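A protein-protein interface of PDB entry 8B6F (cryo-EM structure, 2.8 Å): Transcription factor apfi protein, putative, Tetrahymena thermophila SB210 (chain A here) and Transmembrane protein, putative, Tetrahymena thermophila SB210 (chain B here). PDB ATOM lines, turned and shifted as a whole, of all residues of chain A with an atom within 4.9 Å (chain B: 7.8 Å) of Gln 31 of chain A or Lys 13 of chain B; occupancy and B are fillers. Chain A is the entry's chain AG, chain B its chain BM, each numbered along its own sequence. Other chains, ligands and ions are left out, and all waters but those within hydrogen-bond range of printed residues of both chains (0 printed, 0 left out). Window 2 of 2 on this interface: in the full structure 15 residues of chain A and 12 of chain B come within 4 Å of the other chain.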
ATOM      1  N   LYS A  27      33.536  -1.101  -7.662  1.00  0.00           N
ATOM      2  CA  LYS A  27      32.142  -1.331  -8.026  1.00  0.00           C
ATOM      3  C   LYS A  27      31.315  -0.064  -7.859  1.00  0.00           C
ATOM      4  O   LYS A  27      30.478   0.256  -8.711  1.00  0.00           O
ATOM      5  CB  LYS A  27      31.562  -2.470  -7.191  1.00  0.00           C
ATOM      6  CG  LYS A  27      32.157  -3.832  -7.515  1.00  0.00           C
ATOM      7  CD  LYS A  27      31.462  -4.932  -6.732  1.00  0.00           C
ATOM      8  CE  LYS A  27      32.145  -6.273  -6.918  1.00  0.00           C
ATOM      9  NZ  LYS A  27      33.506  -6.290  -6.329  1.00  0.00           N
ATOM     10  N   SER A  28      31.523   0.667  -6.763  1.00  0.00           N
ATOM     11  CA  SER A  28      30.792   1.916  -6.569  1.00  0.00           C
ATOM     12  C   SER A  28      31.131   2.921  -7.662  1.00  0.00           C
ATOM     13  O   SER A  28      30.243   3.604  -8.185  1.00  0.00           O
ATOM     14  CB  SER A  28      31.102   2.498  -5.190  1.00  0.00           C
ATOM     15  OG  SER A  28      32.486   2.771  -5.051  1.00  0.00           O
ATOM     16  N   LEU A  29      32.413   3.030  -8.016  1.00  0.00           N
ATOM     17  CA  LEU A  29      32.814   3.955  -9.072  1.00  0.00           C
ATOM     18  C   LEU A  29      32.228   3.542 -10.414  1.00  0.00           C
ATOM     19  O   LEU A  29      31.797   4.392 -11.199  1.00  0.00           O
ATOM     20  CB  LEU A  29      34.338   4.038  -9.157  1.00  0.00           C
ATOM     21  CG  LEU A  29      35.050   4.722  -7.986  1.00  0.00           C
ATOM     22  CD1 LEU A  29      36.554   4.624  -8.152  1.00  0.00           C
ATOM     23  CD2 LEU A  29      34.623   6.176  -7.860  1.00  0.00           C
ATOM     24  N   ALA A  30      32.192   2.239 -10.692  1.00  0.00           N
ATOM     25  CA  ALA A  30      31.601   1.777 -11.941  1.00  0.00           C
ATOM     26  C   ALA A  30      30.122   2.126 -12.007  1.00  0.00           C
ATOM     27  O   ALA A  30      29.628   2.571 -13.049  1.00  0.00           O
ATOM     28  CB  ALA A  30      31.805   0.270 -12.091  1.00  0.00           C
ATOM     29  N   GLN A  31      29.396   1.926 -10.907  1.00  0.00           N
ATOM     30  CA  GLN A  31      27.985   2.297 -10.883  1.00  0.00           C
ATOM     31  C   GLN A  31      27.810   3.794 -11.106  1.00  0.00           C
ATOM     32  O   GLN A  31      26.947   4.217 -11.882  1.00  0.00           O
ATOM     33  CB  GLN A  31      27.358   1.877  -9.554  1.00  0.00           C
ATOM     34  CG  GLN A  31      27.064   0.391  -9.449  1.00  0.00           C
ATOM     35  CD  GLN A  31      25.935  -0.045 -10.360  1.00  0.00           C
ATOM     36  OE1 GLN A  31      25.364   0.762 -11.092  1.00  0.00           O
ATOM     37  NE2 GLN A  31      25.602  -1.331 -10.315  1.00  0.00           N
ATOM     38  N   THR A  32      28.620   4.611 -10.430  1.00  0.00           N
ATOM     39  CA  THR A  32      28.517   6.058 -10.593  1.00  0.00           C
ATOM     40  C   THR A  32      28.807   6.469 -12.030  1.00  0.00           C
ATOM     41  O   THR A  32      28.102   7.310 -12.598  1.00  0.00           O
ATOM     42  CB  THR A  32      29.478   6.762  -9.634  1.00  0.00           C
ATOM     43  OG1 THR A  32      29.186   6.374  -8.286  1.00  0.00           O
ATOM     44  CG2 THR A  32      29.349   8.278  -9.753  1.00  0.00           C
ATOM     45  N   GLY A  33      29.842   5.887 -12.635  1.00  0.00           N
ATOM     46  CA  GLY A  33      30.173   6.233 -14.006  1.00  0.00           C
ATOM     47  C   GLY A  33      29.086   5.836 -14.984  1.00  0.00           C
ATOM     48  O   GLY A  33      28.762   6.589 -15.906  1.00  0.00           O
ATOM     49  N   LEU A  34      28.501   4.654 -14.794  1.00  0.00           N
ATOM     50  CA  LEU A  34      27.395   4.234 -15.647  1.00  0.00           C
ATOM     51  C   LEU A  34      26.209   5.178 -15.502  1.00  0.00           C
ATOM     52  O   LEU A  34      25.593   5.568 -16.499  1.00  0.00           O
ATOM     53  CB  LEU A  34      26.992   2.798 -15.312  1.00  0.00           C
ATOM     54  CG  LEU A  34      25.904   2.174 -16.190  1.00  0.00           C
ATOM     55  CD1 LEU A  34      26.361   2.074 -17.635  1.00  0.00           C
ATOM     56  CD2 LEU A  34      25.517   0.808 -15.657  1.00  0.00           C
ATOM     57  N   ASN A  35      25.881   5.567 -14.270  1.00  0.00           N
ATOM     58  CA  ASN A  35      24.782   6.503 -14.063  1.00  0.00           C
ATOM     59  C   ASN A  35      25.054   7.828 -14.763  1.00  0.00           C
ATOM     60  O   ASN A  35      24.149   8.422 -15.359  1.00  0.00           O
ATOM     61  CB  ASN A  35      24.554   6.724 -12.567  1.00  0.00           C
ATOM     62  CG  ASN A  35      24.168   5.452 -11.843  1.00  0.00           C
ATOM     63  OD1 ASN A  35      23.617   4.527 -12.440  1.00  0.00           O
ATOM     64  ND2 ASN A  35      24.453   5.398 -10.547  1.00  0.00           N
ATOM     65  N   ASP A  44      27.225  -4.294 -20.113  1.00  0.00           N
ATOM     66  CA  ASP A  44      27.216  -5.715 -20.423  1.00  0.00           C
ATOM     67  C   ASP A  44      26.064  -6.407 -19.704  1.00  0.00           C
ATOM     68  O   ASP A  44      25.629  -5.988 -18.629  1.00  0.00           O
ATOM     69  CB  ASP A  44      28.544  -6.356 -20.020  1.00  0.00           C
ATOM     70  CG  ASP A  44      29.733  -5.698 -20.691  1.00  0.00           C
ATOM     71  OD1 ASP A  44      29.611  -5.304 -21.868  1.00  0.00           O
ATOM     72  OD2 ASP A  44      30.786  -5.568 -20.037  1.00  0.00           O
ATOM     73  N   PHE B  10      23.430  -7.737  -3.266  1.00  0.00           N
ATOM     74  CA  PHE B  10      23.180  -7.316  -4.636  1.00  0.00           C
ATOM     75  C   PHE B  10      22.795  -5.845  -4.666  1.00  0.00           C
ATOM     76  O   PHE B  10      22.164  -5.330  -3.738  1.00  0.00           O
ATOM     77  CB  PHE B  10      22.063  -8.151  -5.282  1.00  0.00           C
ATOM     78  CG  PHE B  10      22.513  -8.953  -6.471  1.00  0.00           C
ATOM     79  CD1 PHE B  10      22.892  -8.325  -7.644  1.00  0.00           C
ATOM     80  CD2 PHE B  10      22.532 -10.337  -6.419  1.00  0.00           C
ATOM     81  CE1 PHE B  10      23.300  -9.062  -8.742  1.00  0.00           C
ATOM     82  CE2 PHE B  10      22.939 -11.080  -7.512  1.00  0.00           C
ATOM     83  CZ  PHE B  10      23.324 -10.441  -8.675  1.00  0.00           C
ATOM     84  N   VAL B  11      23.184  -5.176  -5.748  1.00  0.00           N
ATOM     85  CA  VAL B  11      22.796  -3.793  -6.009  1.00  0.00           C
ATOM     86  C   VAL B  11      22.070  -3.831  -7.352  1.00  0.00           C
ATOM     87  O   VAL B  11      21.782  -4.919  -7.864  1.00  0.00           O
ATOM     88  CB  VAL B  11      24.027  -2.860  -5.980  1.00  0.00           C
ATOM     89  CG1 VAL B  11      23.654  -1.376  -5.926  1.00  0.00           C
ATOM     90  CG2 VAL B  11      24.903  -3.191  -4.787  1.00  0.00           C
ATOM     91  N   ASP B  12      21.752  -2.667  -7.924  1.00  0.00           N
ATOM     92  CA  ASP B  12      20.926  -2.603  -9.127  1.00  0.00           C
ATOM     93  C   ASP B  12      21.253  -3.709 -10.125  1.00  0.00           C
ATOM     94  O   ASP B  12      20.368  -4.465 -10.538  1.00  0.00           O
ATOM     95  CB  ASP B  12      21.100  -1.233  -9.788  1.00  0.00           C
ATOM     96  CG  ASP B  12      20.669  -0.092  -8.888  1.00  0.00           C
ATOM     97  OD1 ASP B  12      19.713  -0.277  -8.106  1.00  0.00           O
ATOM     98  OD2 ASP B  12      21.291   0.989  -8.957  1.00  0.00           O
ATOM     99  N   LYS B  13      22.519  -3.825 -10.523  1.00  0.00           N
ATOM    100  CA  LYS B  13      22.914  -4.898 -11.427  1.00  0.00           C
ATOM    101  C   LYS B  13      24.169  -5.615 -10.946  1.00  0.00           C
ATOM    102  O   LYS B  13      24.373  -6.791 -11.262  1.00  0.00           O
ATOM    103  CB  LYS B  13      23.139  -4.346 -12.837  1.00  0.00           C
ATOM    104  CG  LYS B  13      21.894  -3.752 -13.488  1.00  0.00           C
ATOM    105  CD  LYS B  13      20.800  -4.790 -13.729  1.00  0.00           C
ATOM    106  CE  LYS B  13      21.209  -5.839 -14.756  1.00  0.00           C
ATOM    107  NZ  LYS B  13      21.581  -5.240 -16.072  1.00  0.00           N
ATOM    108  N   TYR B  14      25.009  -4.929 -10.176  1.00  0.00           N
ATOM    109  CA  TYR B  14      26.301  -5.467  -9.776  1.00  0.00           C
ATOM    110  C   TYR B  14      26.188  -6.195  -8.444  1.00  0.00           C
ATOM    111  O   TYR B  14      25.608  -5.673  -7.486  1.00  0.00           O
ATOM    112  CB  TYR B  14      27.340  -4.348  -9.677  1.00  0.00           C
ATOM    113  CG  TYR B  14      27.688  -3.698 -11.000  1.00  0.00           C
ATOM    114  CD1 TYR B  14      27.269  -4.247 -12.207  1.00  0.00           C
ATOM    115  CD2 TYR B  14      28.451  -2.539 -11.041  1.00  0.00           C
ATOM    116  CE1 TYR B  14      27.591  -3.656 -13.412  1.00  0.00           C
ATOM    117  CE2 TYR B  14      28.777  -1.940 -12.242  1.00  0.00           C
ATOM    118  CZ  TYR B  14      28.345  -2.503 -13.424  1.00  0.00           C
ATOM    119  OH  TYR B  14      28.670  -1.910 -14.620  1.00  0.00           O
ATOM    120  N   ASN B  15      26.754  -7.398  -8.389  1.00  0.00           N
ATOM    121  CA  ASN B  15      26.795  -8.202  -7.170  1.00  0.00           C
ATOM    122  C   ASN B  15      28.043  -7.802  -6.393  1.00  0.00           C
ATOM    123  O   ASN B  15      29.159  -8.184  -6.751  1.00  0.00           O
ATOM    124  CB  ASN B  15      26.791  -9.685  -7.522  1.00  0.00           C
ATOM    125  CG  ASN B  15      26.984 -10.576  -6.315  1.00  0.00           C
ATOM    126  OD1 ASN B  15      26.899 -10.128  -5.175  1.00  0.00           O
ATOM    127  ND2 ASN B  15      27.245 -11.852  -6.563  1.00  0.00           N
ATOM    128  N   PHE B  16      27.854  -7.034  -5.319  1.00  0.00           N
ATOM    129  CA  PHE B  16      28.983  -6.525  -4.550  1.00  0.00           C
ATOM    130  C   PHE B  16      29.699  -7.602  -3.751  1.00  0.00           C
ATOM    131  O   PHE B  16      30.769  -7.325  -3.199  1.00  0.00           O
ATOM    132  CB  PHE B  16      28.515  -5.412  -3.613  1.00  0.00           C
ATOM    133  CG  PHE B  16      28.637  -4.038  -4.204  1.00  0.00           C
ATOM    134  CD1 PHE B  16      28.001  -3.722  -5.393  1.00  0.00           C
ATOM    135  CD2 PHE B  16      29.380  -3.061  -3.566  1.00  0.00           C
ATOM    136  CE1 PHE B  16      28.110  -2.457  -5.937  1.00  0.00           C
ATOM    137  CE2 PHE B  16      29.492  -1.795  -4.104  1.00  0.00           C
ATOM    138  CZ  PHE B  16      28.855  -1.492  -5.291  1.00  0.00           C
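Lys 27 of chain A touches Asn 15 of chain B. Lys 27 of chain A touches Phe 16 of chain B (CB to CZ, 3.4 Å). Ser 28 of chain A touches Phe 16 of chain B. Ala 30 of chain A touches Tyr 14 of chain B. Gln 31 of chain A touches Lys 13 of chain B. Tyr 14 of chain B touches Gln 31 of chain A (CD2 to NE2, 3.2 Å).
O of Ser 28 of chain A sits at hydrogen-bond distance from OG1 of Thr 32 of chain A (3.0 Å). O of Gln 31 of chain A sits close to ND2 of Asn 35 of chain A, 3.1 Å away.
Printed residues of chain B within 4 Å of Gln 31 of chain A: Lys 13 (3.97 Å) and Tyr 14 (3.2 Å). Of chain A, only Gln 31 (3.97 Å) comes within 4 Å of Lys 13 of chain B. Ala 30 of chain A touches one residue of chain B. Printed residues of chain B within 4 Å of Lys 27 of chain A: Asn 15 (3.5 Å) and Phe 16 (3.4 Å). Printed residues of chain A within 4 Å of Phe 16 of chain B: Lys 27 (3.4 Å) and Ser 28 (3.7 Å). Gly 33 of chain A touches none of the printed residues of chain B. The nearest residue of chain B that does not touch Gln 31 of chain A is Asp 12 of chain B (4.5 Å).
Of the 10 printed residues of chain A, 4 touch a printed residue of chain B. Of the 7 printed residues of chain B, 4 touch a printed residue of chain A. Among the printed residues, no Asp or Glu carboxylate lies within 4 Å of a Lys or Arg side-chain nitrogen of the other chain.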
